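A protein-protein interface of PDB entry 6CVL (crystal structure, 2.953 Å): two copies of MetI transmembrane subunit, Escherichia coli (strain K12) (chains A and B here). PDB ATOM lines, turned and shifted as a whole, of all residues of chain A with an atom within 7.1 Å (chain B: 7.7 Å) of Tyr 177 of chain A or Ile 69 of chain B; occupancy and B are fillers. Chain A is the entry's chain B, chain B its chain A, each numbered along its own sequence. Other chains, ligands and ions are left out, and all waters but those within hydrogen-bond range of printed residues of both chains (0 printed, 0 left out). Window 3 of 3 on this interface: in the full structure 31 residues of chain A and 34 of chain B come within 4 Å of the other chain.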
ATOM      1  N   GLY A 159      13.959 -21.655  29.771  1.00  0.00           N
ATOM      2  CA  GLY A 159      13.871 -20.258  30.164  1.00  0.00           C
ATOM      3  C   GLY A 159      14.661 -19.936  31.415  1.00  0.00           C
ATOM      4  O   GLY A 159      15.181 -18.822  31.559  1.00  0.00           O
ATOM      5  N   ALA A 162      17.986 -19.344  30.256  1.00  0.00           N
ATOM      6  CA  ALA A 162      17.961 -18.037  29.607  1.00  0.00           C
ATOM      7  C   ALA A 162      18.179 -16.920  30.623  1.00  0.00           C
ATOM      8  O   ALA A 162      19.033 -16.045  30.434  1.00  0.00           O
ATOM      9  CB  ALA A 162      16.637 -17.843  28.868  1.00  0.00           C
ATOM     10  N   MET A 163      17.416 -16.942  31.715  1.00  0.00           N
ATOM     11  CA  MET A 163      17.569 -15.942  32.766  1.00  0.00           C
ATOM     12  C   MET A 163      18.966 -16.010  33.371  1.00  0.00           C
ATOM     13  O   MET A 163      19.758 -15.072  33.234  1.00  0.00           O
ATOM     14  CB  MET A 163      16.527 -16.135  33.874  1.00  0.00           C
ATOM     15  CG  MET A 163      16.697 -15.194  35.077  1.00  0.00           C
ATOM     16  SD  MET A 163      16.364 -16.007  36.654  1.00  0.00           S
ATOM     17  CE  MET A 163      17.846 -16.997  36.848  1.00  0.00           C
ATOM     18  N   GLY A 171      22.774 -17.667  26.160  1.00  0.00           N
ATOM     19  CA  GLY A 171      21.985 -18.494  25.273  1.00  0.00           C
ATOM     20  C   GLY A 171      20.932 -17.715  24.488  1.00  0.00           C
ATOM     21  O   GLY A 171      20.946 -16.477  24.395  1.00  0.00           O
ATOM     22  N   LEU A 172      19.997 -18.478  23.916  1.00  0.00           N
ATOM     23  CA  LEU A 172      19.008 -17.896  23.016  1.00  0.00           C
ATOM     24  C   LEU A 172      18.157 -16.840  23.708  1.00  0.00           C
ATOM     25  O   LEU A 172      17.795 -15.830  23.096  1.00  0.00           O
ATOM     26  CB  LEU A 172      18.115 -18.989  22.430  1.00  0.00           C
ATOM     27  CG  LEU A 172      18.774 -19.968  21.460  1.00  0.00           C
ATOM     28  CD1 LEU A 172      17.775 -21.041  21.055  1.00  0.00           C
ATOM     29  CD2 LEU A 172      19.317 -19.242  20.238  1.00  0.00           C
ATOM     30  N   GLY A 173      17.815 -17.052  24.979  1.00  0.00           N
ATOM     31  CA  GLY A 173      16.983 -16.080  25.670  1.00  0.00           C
ATOM     32  C   GLY A 173      17.694 -14.755  25.853  1.00  0.00           C
ATOM     33  O   GLY A 173      17.125 -13.684  25.613  1.00  0.00           O
ATOM     34  N   GLN A 174      18.952 -14.809  26.281  1.00  0.00           N
ATOM     35  CA  GLN A 174      19.761 -13.602  26.357  1.00  0.00           C
ATOM     36  C   GLN A 174      19.831 -12.917  25.001  1.00  0.00           C
ATOM     37  O   GLN A 174      19.693 -11.695  24.903  1.00  0.00           O
ATOM     38  CB  GLN A 174      21.157 -13.957  26.851  1.00  0.00           C
ATOM     39  CG  GLN A 174      22.170 -12.828  26.817  1.00  0.00           C
ATOM     40  CD  GLN A 174      21.989 -11.857  27.961  1.00  0.00           C
ATOM     41  OE1 GLN A 174      20.908 -11.758  28.541  1.00  0.00           O
ATOM     42  NE2 GLN A 174      23.054 -11.139  28.300  1.00  0.00           N
ATOM     43  N   ILE A 175      20.063 -13.694  23.941  1.00  0.00           N
ATOM     44  CA  ILE A 175      20.158 -13.107  22.608  1.00  0.00           C
ATOM     45  C   ILE A 175      18.862 -12.386  22.256  1.00  0.00           C
ATOM     46  O   ILE A 175      18.873 -11.260  21.747  1.00  0.00           O
ATOM     47  CB  ILE A 175      20.502 -14.187  21.568  1.00  0.00           C
ATOM     48  CG1 ILE A 175      21.942 -14.661  21.764  1.00  0.00           C
ATOM     49  CG2 ILE A 175      20.295 -13.640  20.163  1.00  0.00           C
ATOM     50  CD1 ILE A 175      22.308 -15.883  20.944  1.00  0.00           C
ATOM     51  N   GLY A 176      17.725 -13.029  22.516  1.00  0.00           N
ATOM     52  CA  GLY A 176      16.450 -12.397  22.236  1.00  0.00           C
ATOM     53  C   GLY A 176      16.267 -11.112  23.017  1.00  0.00           C
ATOM     54  O   GLY A 176      15.770 -10.116  22.488  1.00  0.00           O
ATOM     55  N   TYR A 177      16.672 -11.117  24.289  1.00  0.00           N
ATOM     56  CA  TYR A 177      16.581  -9.905  25.097  1.00  0.00           C
ATOM     57  C   TYR A 177      17.432  -8.794  24.495  1.00  0.00           C
ATOM     58  O   TYR A 177      16.975  -7.655  24.344  1.00  0.00           O
ATOM     59  CB  TYR A 177      17.010 -10.206  26.536  1.00  0.00           C
ATOM     60  CG  TYR A 177      16.881  -9.040  27.503  1.00  0.00           C
ATOM     61  CD1 TYR A 177      15.676  -8.363  27.655  1.00  0.00           C
ATOM     62  CD2 TYR A 177      17.957  -8.639  28.290  1.00  0.00           C
ATOM     63  CE1 TYR A 177      15.553  -7.302  28.547  1.00  0.00           C
ATOM     64  CE2 TYR A 177      17.841  -7.584  29.187  1.00  0.00           C
ATOM     65  CZ  TYR A 177      16.636  -6.920  29.312  1.00  0.00           C
ATOM     66  OH  TYR A 177      16.514  -5.871  30.198  1.00  0.00           O
ATOM     67  N   GLN A 178      18.673  -9.116  24.126  1.00  0.00           N
ATOM     68  CA  GLN A 178      19.605  -8.096  23.659  1.00  0.00           C
ATOM     69  C   GLN A 178      19.274  -7.639  22.245  1.00  0.00           C
ATOM     70  O   GLN A 178      18.946  -6.471  22.017  1.00  0.00           O
ATOM     71  CB  GLN A 178      21.035  -8.634  23.707  1.00  0.00           C
ATOM     72  CG  GLN A 178      21.825  -8.261  24.947  1.00  0.00           C
ATOM     73  CD  GLN A 178      23.318  -8.221  24.678  1.00  0.00           C
ATOM     74  OE1 GLN A 178      23.756  -7.764  23.622  1.00  0.00           O
ATOM     75  NE2 GLN A 178      24.106  -8.702  25.630  1.00  0.00           N
ATOM     76  N   TYR A 179      19.348  -8.548  21.276  1.00  0.00           N
ATOM     77  CA  TYR A 179      19.254  -8.160  19.875  1.00  0.00           C
ATOM     78  C   TYR A 179      17.834  -8.200  19.337  1.00  0.00           C
ATOM     79  O   TYR A 179      17.476  -7.371  18.494  1.00  0.00           O
ATOM     80  CB  TYR A 179      20.155  -9.065  19.033  1.00  0.00           C
ATOM     81  CG  TYR A 179      21.581  -9.094  19.529  1.00  0.00           C
ATOM     82  CD1 TYR A 179      22.521  -8.189  19.054  1.00  0.00           C
ATOM     83  CD2 TYR A 179      21.983 -10.012  20.489  1.00  0.00           C
ATOM     84  CE1 TYR A 179      23.827  -8.210  19.512  1.00  0.00           C
ATOM     85  CE2 TYR A 179      23.284 -10.038  20.953  1.00  0.00           C
ATOM     86  CZ  TYR A 179      24.202  -9.136  20.462  1.00  0.00           C
ATOM     87  OH  TYR A 179      25.499  -9.160  20.922  1.00  0.00           O
ATOM     88  N   GLY A 180      17.009  -9.131  19.811  1.00  0.00           N
ATOM     89  CA  GLY A 180      15.629  -9.167  19.363  1.00  0.00           C
ATOM     90  C   GLY A 180      14.807  -8.036  19.945  1.00  0.00           C
ATOM     91  O   GLY A 180      13.960  -7.455  19.260  1.00  0.00           O
ATOM     92  N   TYR A 181      15.048  -7.700  21.211  1.00  0.00           N
ATOM     93  CA  TYR A 181      14.228  -6.738  21.933  1.00  0.00           C
ATOM     94  C   TYR A 181      14.953  -5.433  22.200  1.00  0.00           C
ATOM     95  O   TYR A 181      14.452  -4.367  21.830  1.00  0.00           O
ATOM     96  CB  TYR A 181      13.745  -7.352  23.256  1.00  0.00           C
ATOM     97  CG  TYR A 181      13.178  -6.336  24.219  1.00  0.00           C
ATOM     98  CD1 TYR A 181      12.006  -5.651  23.925  1.00  0.00           C
ATOM     99  CD2 TYR A 181      13.809  -6.067  25.425  1.00  0.00           C
ATOM    100  CE1 TYR A 181      11.482  -4.723  24.804  1.00  0.00           C
ATOM    101  CE2 TYR A 181      13.293  -5.142  26.310  1.00  0.00           C
ATOM    102  CZ  TYR A 181      12.131  -4.474  25.996  1.00  0.00           C
ATOM    103  OH  TYR A 181      11.617  -3.553  26.879  1.00  0.00           O
ATOM    104  N   ILE A 182      16.129  -5.470  22.826  1.00  0.00           N
ATOM    105  CA  ILE A 182      16.850  -4.234  23.121  1.00  0.00           C
ATOM    106  C   ILE A 182      17.443  -3.768  21.797  1.00  0.00           C
ATOM    107  O   ILE A 182      18.572  -4.126  21.442  1.00  0.00           O
ATOM    108  CB  ILE A 182      17.935  -4.432  24.188  1.00  0.00           C
ATOM    109  CG1 ILE A 182      17.307  -4.771  25.543  1.00  0.00           C
ATOM    110  CG2 ILE A 182      18.753  -3.155  24.327  1.00  0.00           C
ATOM    111  CD1 ILE A 182      18.320  -5.184  26.601  1.00  0.00           C
ATOM    112  N   GLY A 183      16.694  -2.944  21.075  1.00  0.00           N
ATOM    113  CA  GLY A 183      17.081  -2.514  19.748  1.00  0.00           C
ATOM    114  C   GLY A 183      16.253  -3.322  18.771  1.00  0.00           C
ATOM    115  O   GLY A 183      16.467  -4.528  18.615  1.00  0.00           O
ATOM    116  N   MET A 189      14.441 -11.510  16.798  1.00  0.00           N
ATOM    117  CA  MET A 189      13.487 -11.915  17.823  1.00  0.00           C
ATOM    118  C   MET A 189      12.684 -13.122  17.363  1.00  0.00           C
ATOM    119  O   MET A 189      12.554 -14.116  18.090  1.00  0.00           O
ATOM    120  CB  MET A 189      12.562 -10.745  18.156  1.00  0.00           C
ATOM    121  CG  MET A 189      11.592 -10.997  19.303  1.00  0.00           C
ATOM    122  SD  MET A 189      12.295 -10.705  20.935  1.00  0.00           S
ATOM    123  CE  MET A 189      13.117 -12.264  21.252  1.00  0.00           C
ATOM    124  N   VAL A 192      14.781 -16.304  17.347  1.00  0.00           N
ATOM    125  CA  VAL A 192      14.950 -16.828  18.696  1.00  0.00           C
ATOM    126  C   VAL A 192      13.691 -17.563  19.134  1.00  0.00           C
ATOM    127  O   VAL A 192      13.749 -18.695  19.631  1.00  0.00           O
ATOM    128  CB  VAL A 192      15.301 -15.686  19.665  1.00  0.00           C
ATOM    129  CG1 VAL A 192      15.092 -16.120  21.105  1.00  0.00           C
ATOM    130  CG2 VAL A 192      16.735 -15.227  19.444  1.00  0.00           C
ATOM    131  N   ILE B  66       8.261 -18.810  25.478  1.00  0.00           N
ATOM    132  CA  ILE B  66       8.542 -17.373  25.484  1.00  0.00           C
ATOM    133  C   ILE B  66       9.325 -17.036  26.750  1.00  0.00           C
ATOM    134  O   ILE B  66       8.893 -17.405  27.852  1.00  0.00           O
ATOM    135  CB  ILE B  66       7.249 -16.570  25.418  1.00  0.00           C
ATOM    136  CG1 ILE B  66       6.427 -16.963  24.195  1.00  0.00           C
ATOM    137  CG2 ILE B  66       7.561 -15.082  25.358  1.00  0.00           C
ATOM    138  CD1 ILE B  66       5.023 -16.407  24.219  1.00  0.00           C
ATOM    139  N   PRO B  67      10.462 -16.355  26.642  1.00  0.00           N
ATOM    140  CA  PRO B  67      11.132 -15.871  27.850  1.00  0.00           C
ATOM    141  C   PRO B  67      10.232 -14.941  28.645  1.00  0.00           C
ATOM    142  O   PRO B  67       9.343 -14.279  28.103  1.00  0.00           O
ATOM    143  CB  PRO B  67      12.362 -15.142  27.304  1.00  0.00           C
ATOM    144  CG  PRO B  67      12.653 -15.845  26.025  1.00  0.00           C
ATOM    145  CD  PRO B  67      11.312 -16.206  25.447  1.00  0.00           C
ATOM    146  N   PHE B  68      10.483 -14.892  29.956  1.00  0.00           N
ATOM    147  CA  PHE B  68       9.640 -14.105  30.846  1.00  0.00           C
ATOM    148  C   PHE B  68       9.549 -12.665  30.373  1.00  0.00           C
ATOM    149  O   PHE B  68       8.475 -12.054  30.388  1.00  0.00           O
ATOM    150  CB  PHE B  68      10.188 -14.138  32.279  1.00  0.00           C
ATOM    151  CG  PHE B  68      10.906 -15.410  32.641  1.00  0.00           C
ATOM    152  CD1 PHE B  68      10.304 -16.644  32.466  1.00  0.00           C
ATOM    153  CD2 PHE B  68      12.194 -15.367  33.148  1.00  0.00           C
ATOM    154  CE1 PHE B  68      10.973 -17.810  32.799  1.00  0.00           C
ATOM    155  CE2 PHE B  68      12.863 -16.526  33.482  1.00  0.00           C
ATOM    156  CZ  PHE B  68      12.253 -17.747  33.307  1.00  0.00           C
ATOM    157  N   ILE B  69      10.678 -12.110  29.937  1.00  0.00           N
ATOM    158  CA  ILE B  69      10.759 -10.680  29.684  1.00  0.00           C
ATOM    159  C   ILE B  69       9.983 -10.320  28.425  1.00  0.00           C
ATOM    160  O   ILE B  69       9.196  -9.364  28.411  1.00  0.00           O
ATOM    161  CB  ILE B  69      12.234 -10.248  29.586  1.00  0.00           C
ATOM    162  CG1 ILE B  69      13.032 -10.744  30.802  1.00  0.00           C
ATOM    163  CG2 ILE B  69      12.330  -8.738  29.459  1.00  0.00           C
ATOM    164  CD1 ILE B  69      13.568 -12.171  30.682  1.00  0.00           C
ATOM    165  N   ILE B  70      10.206 -11.067  27.344  1.00  0.00           N
ATOM    166  CA  ILE B  70       9.454 -10.821  26.121  1.00  0.00           C
ATOM    167  C   ILE B  70       7.967 -10.955  26.403  1.00  0.00           C
ATOM    168  O   ILE B  70       7.145 -10.197  25.873  1.00  0.00           O
ATOM    169  CB  ILE B  70       9.898 -11.780  25.001  1.00  0.00           C
ATOM    170  CG1 ILE B  70      11.425 -11.902  24.937  1.00  0.00           C
ATOM    171  CG2 ILE B  70       9.355 -11.300  23.658  1.00  0.00           C
ATOM    172  CD1 ILE B  70      12.161 -10.586  24.836  1.00  0.00           C
ATOM    173  N   LEU B  71       7.597 -11.934  27.227  1.00  0.00           N
ATOM    174  CA  LEU B  71       6.196 -12.106  27.582  1.00  0.00           C
ATOM    175  C   LEU B  71       5.664 -10.855  28.260  1.00  0.00           C
ATOM    176  O   LEU B  71       4.640 -10.305  27.852  1.00  0.00           O
ATOM    177  CB  LEU B  71       6.029 -13.324  28.489  1.00  0.00           C
ATOM    178  CG  LEU B  71       4.705 -13.389  29.256  1.00  0.00           C
ATOM    179  CD1 LEU B  71       3.541 -13.538  28.288  1.00  0.00           C
ATOM    180  CD2 LEU B  71       4.719 -14.522  30.271  1.00  0.00           C
ATOM    181  N   LEU B  72       6.349 -10.395  29.306  1.00  0.00           N
ATOM    182  CA  LEU B  72       5.906  -9.202  30.018  1.00  0.00           C
ATOM    183  C   LEU B  72       5.724  -8.043  29.052  1.00  0.00           C
ATOM    184  O   LEU B  72       4.708  -7.339  29.080  1.00  0.00           O
ATOM    185  CB  LEU B  72       6.923  -8.847  31.099  1.00  0.00           C
ATOM    186  CG  LEU B  72       6.436  -8.058  32.315  1.00  0.00           C
ATOM    187  CD1 LEU B  72       7.576  -7.925  33.310  1.00  0.00           C
ATOM    188  CD2 LEU B  72       5.884  -6.698  31.934  1.00  0.00           C
ATOM    189  N   VAL B  73       6.707  -7.842  28.177  1.00  0.00           N
ATOM    190  CA  VAL B  73       6.650  -6.734  27.228  1.00  0.00           C
ATOM    191  C   VAL B  73       5.420  -6.860  26.343  1.00  0.00           C
ATOM    192  O   VAL B  73       4.523  -6.009  26.359  1.00  0.00           O
ATOM    193  CB  VAL B  73       7.935  -6.687  26.385  1.00  0.00           C
ATOM    194  CG1 VAL B  73       7.780  -5.695  25.248  1.00  0.00           C
ATOM    195  CG2 VAL B  73       9.123  -6.326  27.257  1.00  0.00           C
ATOM    196  N   TRP B  74       5.355  -7.939  25.566  1.00  0.00           N
ATOM    197  CA  TRP B  74       4.224  -8.144  24.672  1.00  0.00           C
ATOM    198  C   TRP B  74       2.902  -8.057  25.422  1.00  0.00           C
ATOM    199  O   TRP B  74       1.872  -7.714  24.832  1.00  0.00           O
ATOM    200  CB  TRP B  74       4.378  -9.491  23.973  1.00  0.00           C
ATOM    201  CG  TRP B  74       3.278  -9.804  23.037  1.00  0.00           C
ATOM    202  CD1 TRP B  74       3.158  -9.398  21.741  1.00  0.00           C
ATOM    203  CD2 TRP B  74       2.130 -10.605  23.316  1.00  0.00           C
ATOM    204  NE1 TRP B  74       2.001  -9.898  21.194  1.00  0.00           N
ATOM    205  CE2 TRP B  74       1.352 -10.643  22.142  1.00  0.00           C
ATOM    206  CE3 TRP B  74       1.683 -11.295  24.446  1.00  0.00           C
ATOM    207  CZ2 TRP B  74       0.155 -11.343  22.067  1.00  0.00           C
ATOM    208  CZ3 TRP B  74       0.496 -11.987  24.371  1.00  0.00           C
ATOM    209  CH2 TRP B  74      -0.257 -12.007  23.189  1.00  0.00           C
ATOM    210  N   MET B  75       2.915  -8.349  26.723  1.00  0.00           N
ATOM    211  CA  MET B  75       1.717  -8.240  27.539  1.00  0.00           C
ATOM    212  C   MET B  75       1.376  -6.798  27.862  1.00  0.00           C
ATOM    213  O   MET B  75       0.197  -6.470  28.027  1.00  0.00           O
ATOM    214  CB  MET B  75       1.912  -9.004  28.848  1.00  0.00           C
ATOM    215  CG  MET B  75       1.988 -10.513  28.708  1.00  0.00           C
ATOM    216  SD  MET B  75       0.371 -11.294  28.733  1.00  0.00           S
ATOM    217  CE  MET B  75      -0.215 -10.777  30.347  1.00  0.00           C
ATOM    218  N   ILE B  76       2.392  -5.947  27.970  1.00  0.00           N
ATOM    219  CA  ILE B  76       2.240  -4.576  28.449  1.00  0.00           C
ATOM    220  C   ILE B  76       0.912  -3.971  28.014  1.00  0.00           C
ATOM    221  O   ILE B  76       0.138  -3.516  28.868  1.00  0.00           O
ATOM    222  CB  ILE B  76       3.405  -3.696  27.966  1.00  0.00           C
ATOM    223  CG1 ILE B  76       4.680  -4.029  28.737  1.00  0.00           C
ATOM    224  CG2 ILE B  76       3.051  -2.221  28.110  1.00  0.00           C
ATOM    225  CD1 ILE B  76       5.922  -3.414  28.132  1.00  0.00           C
ATOM    226  N   PRO B  95       1.438 -10.510  33.979  1.00  0.00           N
ATOM    227  CA  PRO B  95       2.377 -11.342  33.216  1.00  0.00           C
ATOM    228  C   PRO B  95       2.862 -12.541  33.995  1.00  0.00           C
ATOM    229  O   PRO B  95       3.091 -13.597  33.401  1.00  0.00           O
ATOM    230  CB  PRO B  95       3.527 -10.380  32.895  1.00  0.00           C
ATOM    231  CG  PRO B  95       2.959  -9.022  33.077  1.00  0.00           C
ATOM    232  CD  PRO B  95       1.953  -9.147  34.166  1.00  0.00           C
ATOM    233  N   TYR B 160       9.925 -16.509  41.571  1.00  0.00           N
ATOM    234  CA  TYR B 160       9.525 -16.061  40.243  1.00  0.00           C
ATOM    235  C   TYR B 160       8.976 -14.640  40.294  1.00  0.00           C
ATOM    236  O   TYR B 160       9.278 -13.814  39.422  1.00  0.00           O
ATOM    237  CB  TYR B 160       8.497 -17.039  39.678  1.00  0.00           C
ATOM    238  CG  TYR B 160       8.292 -16.966  38.188  1.00  0.00           C
ATOM    239  CD1 TYR B 160       9.095 -17.690  37.317  1.00  0.00           C
ATOM    240  CD2 TYR B 160       7.277 -16.195  37.654  1.00  0.00           C
ATOM    241  CE1 TYR B 160       8.895 -17.629  35.950  1.00  0.00           C
ATOM    242  CE2 TYR B 160       7.070 -16.126  36.294  1.00  0.00           C
ATOM    243  CZ  TYR B 160       7.879 -16.844  35.446  1.00  0.00           C
ATOM    244  OH  TYR B 160       7.661 -16.770  34.092  1.00  0.00           O
ATOM    245  N   MET B 163      11.812 -12.142  40.830  1.00  0.00           N
ATOM    246  CA  MET B 163      12.383 -11.776  39.540  1.00  0.00           C
ATOM    247  C   MET B 163      11.472 -10.809  38.792  1.00  0.00           C
ATOM    248  O   MET B 163      11.818  -9.638  38.599  1.00  0.00           O
ATOM    249  CB  MET B 163      12.620 -13.027  38.683  1.00  0.00           C
ATOM    250  CG  MET B 163      13.120 -12.750  37.263  1.00  0.00           C
ATOM    251  SD  MET B 163      12.370 -13.848  36.047  1.00  0.00           S
ATOM    252  CE  MET B 163      10.730 -13.147  35.910  1.00  0.00           C
ATOM    253  N   GLY B 164      10.294 -11.286  38.391  1.00  0.00           N
ATOM    254  CA  GLY B 164       9.450 -10.542  37.475  1.00  0.00           C
ATOM    255  C   GLY B 164       8.872  -9.259  38.030  1.00  0.00           C
ATOM    256  O   GLY B 164       8.245  -8.510  37.272  1.00  0.00           O
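Among the printed residues, pairs that only touch across the chains: Gly 159 of chain A with Phe 68 of chain B (3.6 Å), Tyr 177 of chain A with Ile 69 of chain B (3.6 Å), Met 163 of chain A with Phe 68 of chain B (3.7 Å), Tyr 181 of chain A with Val 73 of chain B (3.7 Å), Met 189 of chain A with Ile 70 of chain B (3.9 Å) and Tyr 181 of chain A with Ile 70 of chain B (3.9 Å).
1 position is printed for both chains. Of the 6 pairs that touch across the chains among the printed residues, none has its exchanged pair printed and touching as well.
Of the 18 printed residues of chain A, 5 touch a printed residue of chain B. Hydrophobic or aromatic side chains of chain A within 4 Å of the printed part of chain B: Met 163, Tyr 177, Tyr 181 and Met 189. Of the 15 printed residues of chain B, 4 touch a printed residue of chain A. Hydrophobic or aromatic side chains of chain B that line the printed part of chain A: Phe 68, Ile 69, Ile 70 and Val 73. Among the printed residues, 6 pairs touch across the chains. Among the printed residues, no Asp or Glu carboxylate lies within 4 Å of a Lys or Arg side-chain nitrogen of the other chain.
Ile 69 of chain B touches one residue of chain A. Printed residues of chain B within 4 Å of Gly 159 of chain A: Phe 68. Of the printed residues of chain A, Phe 68 of chain B touches Gly 159 (3.6 Å) and Met 163 (3.7 Å). The nearest residue of chain B that does not touch Tyr 177 of chain A is Ile 70 of chain B (4.5 Å). The nearest printed residue of chain B that does not touch Gly 159 of chain A is Pro 67 of chain B (5.7 Å).
The backbone carbonyl oxygen of Tyr 177 of chain A lies within hydrogen-bond range of the backbone NH of Ile 182 of chain A, 2.8 Å away. The backbone carbonyl oxygen (O) of Gly 176 of chain A lies within hydrogen-bond range of the backbone NH (N) of Tyr 181 of chain A (2.8 Å).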
